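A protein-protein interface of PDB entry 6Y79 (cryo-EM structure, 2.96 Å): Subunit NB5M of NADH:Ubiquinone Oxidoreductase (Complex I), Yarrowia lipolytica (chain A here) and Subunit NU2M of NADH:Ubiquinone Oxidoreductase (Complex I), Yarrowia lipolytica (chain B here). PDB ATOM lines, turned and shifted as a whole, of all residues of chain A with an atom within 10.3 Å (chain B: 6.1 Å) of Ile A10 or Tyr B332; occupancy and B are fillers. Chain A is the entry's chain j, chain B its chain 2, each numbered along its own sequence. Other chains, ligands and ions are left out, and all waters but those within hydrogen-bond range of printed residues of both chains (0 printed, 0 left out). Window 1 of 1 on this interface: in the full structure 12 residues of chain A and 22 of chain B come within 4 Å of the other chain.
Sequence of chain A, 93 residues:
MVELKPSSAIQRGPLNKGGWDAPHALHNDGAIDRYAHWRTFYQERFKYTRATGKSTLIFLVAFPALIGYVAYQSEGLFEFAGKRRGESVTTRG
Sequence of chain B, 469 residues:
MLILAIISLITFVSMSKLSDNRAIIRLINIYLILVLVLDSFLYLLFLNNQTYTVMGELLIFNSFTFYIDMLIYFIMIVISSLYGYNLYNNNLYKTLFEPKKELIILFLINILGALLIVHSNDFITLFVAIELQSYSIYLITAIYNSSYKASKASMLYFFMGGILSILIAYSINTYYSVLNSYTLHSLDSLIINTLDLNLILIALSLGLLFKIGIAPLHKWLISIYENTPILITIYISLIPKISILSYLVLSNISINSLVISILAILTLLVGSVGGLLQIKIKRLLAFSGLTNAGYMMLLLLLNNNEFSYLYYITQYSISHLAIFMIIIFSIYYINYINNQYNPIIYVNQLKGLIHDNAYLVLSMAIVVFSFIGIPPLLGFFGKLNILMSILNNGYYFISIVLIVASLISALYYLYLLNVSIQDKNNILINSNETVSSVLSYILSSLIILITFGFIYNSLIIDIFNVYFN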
ATOM      1  N   LYS A   5      14.690   8.099  -0.345  1.00  0.00           N
ATOM      2  CA  LYS A   5      15.081   7.015  -1.218  1.00  0.00           C
ATOM      3  C   LYS A   5      16.236   7.528  -2.063  1.00  0.00           C
ATOM      4  O   LYS A   5      16.120   8.619  -2.640  1.00  0.00           O
ATOM      5  CB  LYS A   5      13.928   6.600  -2.134  1.00  0.00           C
ATOM      6  CG  LYS A   5      12.648   6.286  -1.432  1.00  0.00           C
ATOM      7  CD  LYS A   5      12.702   4.913  -0.827  1.00  0.00           C
ATOM      8  CE  LYS A   5      11.325   4.493  -0.389  1.00  0.00           C
ATOM      9  NZ  LYS A   5      10.913   5.293   0.793  1.00  0.00           N
ATOM     10  N   PRO A   6      17.337   6.778  -2.181  1.00  0.00           N
ATOM     11  CA  PRO A   6      18.415   7.157  -3.104  1.00  0.00           C
ATOM     12  C   PRO A   6      17.923   7.275  -4.537  1.00  0.00           C
ATOM     13  O   PRO A   6      16.938   6.645  -4.923  1.00  0.00           O
ATOM     14  CB  PRO A   6      19.424   6.015  -2.954  1.00  0.00           C
ATOM     15  CG  PRO A   6      18.644   4.892  -2.336  1.00  0.00           C
ATOM     16  CD  PRO A   6      17.661   5.549  -1.442  1.00  0.00           C
ATOM     17  N   SER A   7      18.650   8.078  -5.319  1.00  0.00           N
ATOM     18  CA  SER A   7      18.125   8.834  -6.452  1.00  0.00           C
ATOM     19  C   SER A   7      17.494   7.944  -7.526  1.00  0.00           C
ATOM     20  O   SER A   7      17.767   6.751  -7.641  1.00  0.00           O
ATOM     21  CB  SER A   7      19.235   9.672  -7.081  1.00  0.00           C
ATOM     22  OG  SER A   7      19.634  10.715  -6.211  1.00  0.00           O
ATOM     23  N   SER A   8      16.624   8.561  -8.324  1.00  0.00           N
ATOM     24  CA  SER A   8      16.009   7.884  -9.457  1.00  0.00           C
ATOM     25  C   SER A   8      16.995   7.598 -10.576  1.00  0.00           C
ATOM     26  O   SER A   8      16.681   6.803 -11.469  1.00  0.00           O
ATOM     27  CB  SER A   8      14.865   8.733 -10.009  1.00  0.00           C
ATOM     28  OG  SER A   8      15.367   9.825 -10.763  1.00  0.00           O
ATOM     29  N   ALA A   9      18.180   8.199 -10.535  1.00  0.00           N
ATOM     30  CA  ALA A   9      19.088   8.222 -11.665  1.00  0.00           C
ATOM     31  C   ALA A   9      20.341   7.413 -11.366  1.00  0.00           C
ATOM     32  O   ALA A   9      21.458   7.865 -11.624  1.00  0.00           O
ATOM     33  CB  ALA A   9      19.438   9.664 -12.001  1.00  0.00           C
ATOM     34  N   ILE A  10      20.165   6.220 -10.809  1.00  0.00           N
ATOM     35  CA  ILE A  10      21.266   5.386 -10.348  1.00  0.00           C
ATOM     36  C   ILE A  10      21.656   4.338 -11.388  1.00  0.00           C
ATOM     37  O   ILE A  10      22.840   4.161 -11.678  1.00  0.00           O
ATOM     38  CB  ILE A  10      20.927   4.733  -8.991  1.00  0.00           C
ATOM     39  CG1 ILE A  10      20.848   5.805  -7.911  1.00  0.00           C
ATOM     40  CG2 ILE A  10      21.964   3.707  -8.587  1.00  0.00           C
ATOM     41  CD1 ILE A  10      22.176   6.337  -7.473  1.00  0.00           C
ATOM     42  N   GLN A  11      20.662   3.648 -11.967  1.00  0.00           N
ATOM     43  CA  GLN A  11      20.849   2.525 -12.900  1.00  0.00           C
ATOM     44  C   GLN A  11      21.813   1.493 -12.320  1.00  0.00           C
ATOM     45  O   GLN A  11      22.882   1.246 -12.866  1.00  0.00           O
ATOM     46  CB  GLN A  11      21.317   2.999 -14.288  1.00  0.00           C
ATOM     47  CG  GLN A  11      21.077   2.029 -15.466  1.00  0.00           C
ATOM     48  CD  GLN A  11      22.309   1.243 -15.895  1.00  0.00           C
ATOM     49  OE1 GLN A  11      23.447   1.653 -15.613  1.00  0.00           O
ATOM     50  NE2 GLN A  11      22.099   0.142 -16.609  1.00  0.00           N
ATOM     51  N   ARG A  12      21.512   0.959 -11.147  1.00  0.00           N
ATOM     52  CA  ARG A  12      22.471   0.016 -10.597  1.00  0.00           C
ATOM     53  C   ARG A  12      22.145  -1.392 -11.061  1.00  0.00           C
ATOM     54  O   ARG A  12      20.986  -1.741 -11.288  1.00  0.00           O
ATOM     55  CB  ARG A  12      22.525   0.098  -9.081  1.00  0.00           C
ATOM     56  CG  ARG A  12      21.247  -0.149  -8.371  1.00  0.00           C
ATOM     57  CD  ARG A  12      21.538  -0.428  -6.922  1.00  0.00           C
ATOM     58  NE  ARG A  12      21.889   0.781  -6.181  1.00  0.00           N
ATOM     59  CZ  ARG A  12      23.117   1.068  -5.765  1.00  0.00           C
ATOM     60  NH1 ARG A  12      24.113   0.243  -6.039  1.00  0.00           N
ATOM     61  NH2 ARG A  12      23.355   2.180  -5.087  1.00  0.00           N
ATOM     62  N   GLY A  13      23.187  -2.193 -11.231  1.00  0.00           N
ATOM     63  CA  GLY A  13      23.044  -3.512 -11.786  1.00  0.00           C
ATOM     64  C   GLY A  13      24.052  -4.478 -11.206  1.00  0.00           C
ATOM     65  O   GLY A  13      24.929  -4.099 -10.427  1.00  0.00           O
ATOM     66  N   PRO A  14      23.954  -5.751 -11.586  1.00  0.00           N
ATOM     67  CA  PRO A  14      24.733  -6.785 -10.898  1.00  0.00           C
ATOM     68  C   PRO A  14      26.203  -6.798 -11.295  1.00  0.00           C
ATOM     69  O   PRO A  14      26.587  -6.381 -12.389  1.00  0.00           O
ATOM     70  CB  PRO A  14      24.036  -8.084 -11.311  1.00  0.00           C
ATOM     71  CG  PRO A  14      23.379  -7.764 -12.601  1.00  0.00           C
ATOM     72  CD  PRO A  14      22.982  -6.326 -12.532  1.00  0.00           C
ATOM     73  N   TYR B  88      24.285  17.503  -4.467  1.00  0.00           N
ATOM     74  CA  TYR B  88      23.644  17.285  -5.753  1.00  0.00           C
ATOM     75  C   TYR B  88      22.423  18.180  -5.830  1.00  0.00           C
ATOM     76  O   TYR B  88      21.946  18.712  -4.824  1.00  0.00           O
ATOM     77  CB  TYR B  88      23.180  15.835  -5.974  1.00  0.00           C
ATOM     78  CG  TYR B  88      24.215  14.731  -6.064  1.00  0.00           C
ATOM     79  CD1 TYR B  88      25.532  14.935  -5.757  1.00  0.00           C
ATOM     80  CD2 TYR B  88      23.863  13.482  -6.494  1.00  0.00           C
ATOM     81  CE1 TYR B  88      26.437  13.956  -5.828  1.00  0.00           C
ATOM     82  CE2 TYR B  88      24.802  12.501  -6.618  1.00  0.00           C
ATOM     83  CZ  TYR B  88      26.093  12.752  -6.271  1.00  0.00           C
ATOM     84  OH  TYR B  88      27.081  11.811  -6.352  1.00  0.00           O
ATOM     85  N   ASN B  90      19.280  17.245  -6.272  1.00  0.00           N
ATOM     86  CA  ASN B  90      18.149  16.348  -6.125  1.00  0.00           C
ATOM     87  C   ASN B  90      17.111  17.023  -5.249  1.00  0.00           C
ATOM     88  O   ASN B  90      17.376  18.037  -4.605  1.00  0.00           O
ATOM     89  CB  ASN B  90      18.565  15.016  -5.491  1.00  0.00           C
ATOM     90  CG  ASN B  90      19.454  14.196  -6.382  1.00  0.00           C
ATOM     91  OD1 ASN B  90      20.505  13.726  -5.961  1.00  0.00           O
ATOM     92  ND2 ASN B  90      19.040  14.019  -7.626  1.00  0.00           N
ATOM     93  N   TYR B  93      18.872  15.863  -1.528  1.00  0.00           N
ATOM     94  CA  TYR B  93      19.896  16.518  -0.712  1.00  0.00           C
ATOM     95  C   TYR B  93      19.463  17.888  -0.266  1.00  0.00           C
ATOM     96  O   TYR B  93      20.106  18.447   0.612  1.00  0.00           O
ATOM     97  CB  TYR B  93      21.247  16.614  -1.463  1.00  0.00           C
ATOM     98  CG  TYR B  93      21.916  15.287  -1.579  1.00  0.00           C
ATOM     99  CD1 TYR B  93      22.011  14.421  -0.495  1.00  0.00           C
ATOM    100  CD2 TYR B  93      22.403  14.881  -2.769  1.00  0.00           C
ATOM    101  CE1 TYR B  93      22.627  13.202  -0.635  1.00  0.00           C
ATOM    102  CE2 TYR B  93      23.017  13.671  -2.929  1.00  0.00           C
ATOM    103  CZ  TYR B  93      23.122  12.838  -1.858  1.00  0.00           C
ATOM    104  OH  TYR B  93      23.727  11.632  -2.015  1.00  0.00           O
ATOM    105  N   ILE B 328      30.469  12.025   4.002  1.00  0.00           N
ATOM    106  CA  ILE B 328      29.410  12.806   3.366  1.00  0.00           C
ATOM    107  C   ILE B 328      29.191  12.310   1.946  1.00  0.00           C
ATOM    108  O   ILE B 328      28.052  12.164   1.487  1.00  0.00           O
ATOM    109  CB  ILE B 328      29.736  14.313   3.389  1.00  0.00           C
ATOM    110  CG1 ILE B 328      29.766  14.853   4.809  1.00  0.00           C
ATOM    111  CG2 ILE B 328      28.715  15.110   2.622  1.00  0.00           C
ATOM    112  CD1 ILE B 328      28.488  14.697   5.543  1.00  0.00           C
ATOM    113  N   PHE B 329      30.276  12.012   1.235  1.00  0.00           N
ATOM    114  CA  PHE B 329      30.157  11.606  -0.165  1.00  0.00           C
ATOM    115  C   PHE B 329      29.609  10.202  -0.339  1.00  0.00           C
ATOM    116  O   PHE B 329      29.076   9.888  -1.405  1.00  0.00           O
ATOM    117  CB  PHE B 329      31.504  11.657  -0.876  1.00  0.00           C
ATOM    118  CG  PHE B 329      31.947  13.024  -1.248  1.00  0.00           C
ATOM    119  CD1 PHE B 329      31.231  14.131  -0.870  1.00  0.00           C
ATOM    120  CD2 PHE B 329      33.069  13.198  -2.016  1.00  0.00           C
ATOM    121  CE1 PHE B 329      31.638  15.368  -1.210  1.00  0.00           C
ATOM    122  CE2 PHE B 329      33.473  14.453  -2.375  1.00  0.00           C
ATOM    123  CZ  PHE B 329      32.751  15.538  -1.970  1.00  0.00           C
ATOM    124  N   SER B 330      29.760   9.347   0.665  1.00  0.00           N
ATOM    125  CA  SER B 330      29.302   7.973   0.528  1.00  0.00           C
ATOM    126  C   SER B 330      27.798   7.807   0.695  1.00  0.00           C
ATOM    127  O   SER B 330      27.311   6.683   0.555  1.00  0.00           O
ATOM    128  CB  SER B 330      30.029   7.098   1.535  1.00  0.00           C
ATOM    129  OG  SER B 330      31.411   7.103   1.260  1.00  0.00           O
ATOM    130  N   ILE B 331      27.056   8.881   0.979  1.00  0.00           N
ATOM    131  CA  ILE B 331      25.617   8.795   1.216  1.00  0.00           C
ATOM    132  C   ILE B 331      24.871   8.506  -0.080  1.00  0.00           C
ATOM    133  O   ILE B 331      23.797   7.893  -0.072  1.00  0.00           O
ATOM    134  CB  ILE B 331      25.150  10.095   1.898  1.00  0.00           C
ATOM    135  CG1 ILE B 331      25.876  10.260   3.221  1.00  0.00           C
ATOM    136  CG2 ILE B 331      23.660  10.120   2.182  1.00  0.00           C
ATOM    137  CD1 ILE B 331      25.718  11.609   3.819  1.00  0.00           C
ATOM    138  N   TYR B 332      25.453   8.878  -1.216  1.00  0.00           N
ATOM    139  CA  TYR B 332      24.850   8.614  -2.513  1.00  0.00           C
ATOM    140  C   TYR B 332      24.782   7.135  -2.856  1.00  0.00           C
ATOM    141  O   TYR B 332      23.962   6.740  -3.689  1.00  0.00           O
ATOM    142  CB  TYR B 332      25.645   9.346  -3.576  1.00  0.00           C
ATOM    143  CG  TYR B 332      25.027   9.334  -4.938  1.00  0.00           C
ATOM    144  CD1 TYR B 332      23.682   9.619  -5.113  1.00  0.00           C
ATOM    145  CD2 TYR B 332      25.788   9.031  -6.052  1.00  0.00           C
ATOM    146  CE1 TYR B 332      23.118   9.611  -6.367  1.00  0.00           C
ATOM    147  CE2 TYR B 332      25.245   9.037  -7.302  1.00  0.00           C
ATOM    148  CZ  TYR B 332      23.912   9.333  -7.457  1.00  0.00           C
ATOM    149  OH  TYR B 332      23.359   9.321  -8.712  1.00  0.00           O
ATOM    150  N   TYR B 333      25.595   6.307  -2.216  1.00  0.00           N
ATOM    151  CA  TYR B 333      25.760   4.927  -2.616  1.00  0.00           C
ATOM    152  C   TYR B 333      25.188   3.939  -1.622  1.00  0.00           C
ATOM    153  O   TYR B 333      25.246   2.734  -1.871  1.00  0.00           O
ATOM    154  CB  TYR B 333      27.240   4.647  -2.840  1.00  0.00           C
ATOM    155  CG  TYR B 333      27.825   5.540  -3.889  1.00  0.00           C
ATOM    156  CD1 TYR B 333      27.572   5.306  -5.218  1.00  0.00           C
ATOM    157  CD2 TYR B 333      28.609   6.628  -3.549  1.00  0.00           C
ATOM    158  CE1 TYR B 333      28.092   6.110  -6.184  1.00  0.00           C
ATOM    159  CE2 TYR B 333      29.131   7.447  -4.513  1.00  0.00           C
ATOM    160  CZ  TYR B 333      28.865   7.179  -5.831  1.00  0.00           C
ATOM    161  OH  TYR B 333      29.375   7.982  -6.813  1.00  0.00           O
ATOM    162  N   ILE B 334      24.643   4.399  -0.519  1.00  0.00           N
ATOM    163  CA  ILE B 334      24.082   3.489   0.466  1.00  0.00           C
ATOM    164  C   ILE B 334      22.674   3.093   0.041  1.00  0.00           C
ATOM    165  O   ILE B 334      21.971   3.841  -0.643  1.00  0.00           O
ATOM    166  CB  ILE B 334      24.113   4.121   1.871  1.00  0.00           C
ATOM    167  CG1 ILE B 334      23.246   5.370   1.935  1.00  0.00           C
ATOM    168  CG2 ILE B 334      25.526   4.481   2.244  1.00  0.00           C
ATOM    169  CD1 ILE B 334      23.178   5.987   3.293  1.00  0.00           C
ATOM    170  N   LEU B 428      26.833   0.305  -9.187  1.00  0.00           N
ATOM    171  CA  LEU B 428      26.441   1.391 -10.073  1.00  0.00           C
ATOM    172  C   LEU B 428      27.159   1.247 -11.407  1.00  0.00           C
ATOM    173  O   LEU B 428      28.264   0.722 -11.481  1.00  0.00           O
ATOM    174  CB  LEU B 428      26.770   2.751  -9.450  1.00  0.00           C
ATOM    175  CG  LEU B 428      26.380   4.089 -10.074  1.00  0.00           C
ATOM    176  CD1 LEU B 428      26.067   5.014  -8.942  1.00  0.00           C
ATOM    177  CD2 LEU B 428      27.484   4.708 -10.946  1.00  0.00           C
ATOM    178  N   ILE B 429      26.508   1.685 -12.474  1.00  0.00           N
ATOM    179  CA  ILE B 429      27.114   1.744 -13.792  1.00  0.00           C
ATOM    180  C   ILE B 429      27.059   3.156 -14.363  1.00  0.00           C
ATOM    181  O   ILE B 429      28.038   3.641 -14.940  1.00  0.00           O
ATOM    182  CB  ILE B 429      26.448   0.722 -14.751  1.00  0.00           C
ATOM    183  CG1 ILE B 429      26.689  -0.716 -14.291  1.00  0.00           C
ATOM    184  CG2 ILE B 429      26.981   0.855 -16.154  1.00  0.00           C
ATOM    185  CD1 ILE B 429      25.531  -1.349 -13.561  1.00  0.00           C
ATOM    186  N   ASN B 430      25.934   3.840 -14.171  1.00  0.00           N
ATOM    187  CA  ASN B 430      25.616   5.040 -14.935  1.00  0.00           C
ATOM    188  C   ASN B 430      24.749   5.955 -14.106  1.00  0.00           C
ATOM    189  O   ASN B 430      23.569   5.657 -13.916  1.00  0.00           O
ATOM    190  CB  ASN B 430      24.867   4.639 -16.232  1.00  0.00           C
ATOM    191  CG  ASN B 430      24.290   5.831 -16.994  1.00  0.00           C
ATOM    192  OD1 ASN B 430      23.253   6.363 -16.616  1.00  0.00           O
ATOM    193  ND2 ASN B 430      24.932   6.218 -18.090  1.00  0.00           N
ATOM    194  N   SER B 431      25.302   7.065 -13.662  1.00  0.00           N
ATOM    195  CA  SER B 431      24.518   8.017 -12.898  1.00  0.00           C
ATOM    196  C   SER B 431      24.513   9.404 -13.524  1.00  0.00           C
ATOM    197  O   SER B 431      25.542   9.918 -13.962  1.00  0.00           O
ATOM    198  CB  SER B 431      24.977   8.056 -11.442  1.00  0.00           C
ATOM    199  OG  SER B 431      24.360   6.952 -10.812  1.00  0.00           O
ATOM    200  N   ASN B 432      23.322   9.992 -13.565  1.00  0.00           N
ATOM    201  CA  ASN B 432      23.026  11.152 -14.388  1.00  0.00           C
ATOM    202  C   ASN B 432      23.612  12.415 -13.781  1.00  0.00           C
ATOM    203  O   ASN B 432      24.214  13.225 -14.488  1.00  0.00           O
ATOM    204  CB  ASN B 432      21.507  11.244 -14.542  1.00  0.00           C
ATOM    205  CG  ASN B 432      21.058  12.427 -15.344  1.00  0.00           C
ATOM    206  OD1 ASN B 432      21.424  12.580 -16.511  1.00  0.00           O
ATOM    207  ND2 ASN B 432      20.239  13.268 -14.734  1.00  0.00           N
ATOM    208  N   GLU B 433      23.462  12.595 -12.476  1.00  0.00           N
ATOM    209  CA  GLU B 433      23.905  13.824 -11.845  1.00  0.00           C
ATOM    210  C   GLU B 433      25.207  13.616 -11.081  1.00  0.00           C
ATOM    211  O   GLU B 433      25.540  12.510 -10.642  1.00  0.00           O
ATOM    212  CB  GLU B 433      22.821  14.390 -10.932  1.00  0.00           C
ATOM    213  CG  GLU B 433      22.553  13.601  -9.704  1.00  0.00           C
ATOM    214  CD  GLU B 433      21.457  12.595  -9.873  1.00  0.00           C
ATOM    215  OE1 GLU B 433      21.038  12.374 -11.020  1.00  0.00           O
ATOM    216  OE2 GLU B 433      21.006  12.030  -8.858  1.00  0.00           O
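The side-chain hydroxyl of Ser A7 is in hydrogen-bond range of the side-chain amide oxygen of Asn B90.
OE2 of Glu B433 lies within hydrogen-bond range of OG of Ser A7, at 3.3 Å.
The backbone carbonyl oxygen (O) of Ile A10 sits close to the backbone carbonyl oxygen (O) of Asn B430 (2.8 Å).
The backbone NH of Asn B432 lies within hydrogen-bond range of the backbone carbonyl oxygen of Ala A9 (3.4 Å).
The backbone carbonyl oxygen of Ile A10 lies within hydrogen-bond range of the side-chain hydroxyl of Ser B431 (3.3 Å).
The side-chain hydroxyl of Ser B431 lies within hydrogen-bond range of the backbone carbonyl oxygen of Ala A9 (3.1 Å).
The side-chain carboxylate (OE2) of Glu B433 is in hydrogen-bond range of the side-chain amide nitrogen (ND2) of Asn B90 (3.1 Å).
The side-chain hydroxyl (OH) of Tyr B93 lies close to the backbone NH (N) of Tyr B332 (3.3 Å).
The side-chain hydroxyl (OH) of Tyr B332 is in hydrogen-bond range of the side-chain hydroxyl (OG) of Ser B431 (3.3 Å).
O of Ile B334 touches CG of Pro A6, 3.9 Å away.
Tyr B332 touches Ser A7 (CE1 to OG, 3.7 Å).
Tyr B332 touches Ala A9 (OH to O, 3.8 Å).
Asn B430 touches Ala A9.
Ile A10 touches Tyr B332.
CG of Leu B428 touches O of Ile A10 (3.9 Å).
CB of Ile B429 touches OE1 of Gln A11, 3.3 Å away.
Gln A11 touches Asn B430 (OE1 to CB, 3.4 Å).
Tyr B333 touches Arg A12.
N of Gly A13 touches CD1 of Ile B429, at 3.4 Å.
Printed residues of chain B within 4 Å of Ile A10: Tyr B332 (3.4 Å), Leu B428 (3.9 Å), Asn B430 (2.8 Å) and Ser B431 (3.3 Å).
Tyr B332 touches just these residues of chain A: Ser A7, Ala A9 and Ile A10.
No residue of chain A comes within 4 Å of Ile B331.
Of the printed residues of chain A, Tyr B333 touches Arg A12.
Ile B334 touches just one residue of chain A: Pro A6 (3.9 Å).
Of the printed residues of chain A, Glu B433 touches Ser A7 and Ala A9.
Of the printed residues of chain A, Asn B430 touches Ala A9, Ile A10 and Gln A11.
Of the printed residues of chain B, Pro A6 touches Ile B334.
Of the printed residues of chain A, Ile B429 touches Gln A11 (3.3 Å) and Gly A13 (3.4 Å).
Of the printed residues of chain B, Ala A9 touches Tyr B332 (3.8 Å), Asn B430 (3.8 Å), Ser B431 (3.1 Å), Asn B432 (3.4 Å) and Glu B433 (3.3 Å).
Printed residues of chain A within 4 Å of Leu B428: Ile A10 (3.9 Å).
Tyr B88 touches none of the printed residues of chain A.
Phe B329 touches none of the printed residues of chain A.
Of the 16 printed residues of chain B, 10 touch a printed residue of chain A.
Of the 10 printed residues of chain A, 7 touch a printed residue of chain B.
Hydrophobic or aromatic side chains of chain A within 4 Å of the printed part of chain B: Pro A6, Ala A9 and Ile A10.
Among the printed residues, 17 pairs touch across the chains.
Among the printed residues, no Asp or Glu carboxylate lies within 4 Å of a Lys or Arg side-chain nitrogen of the other chain.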
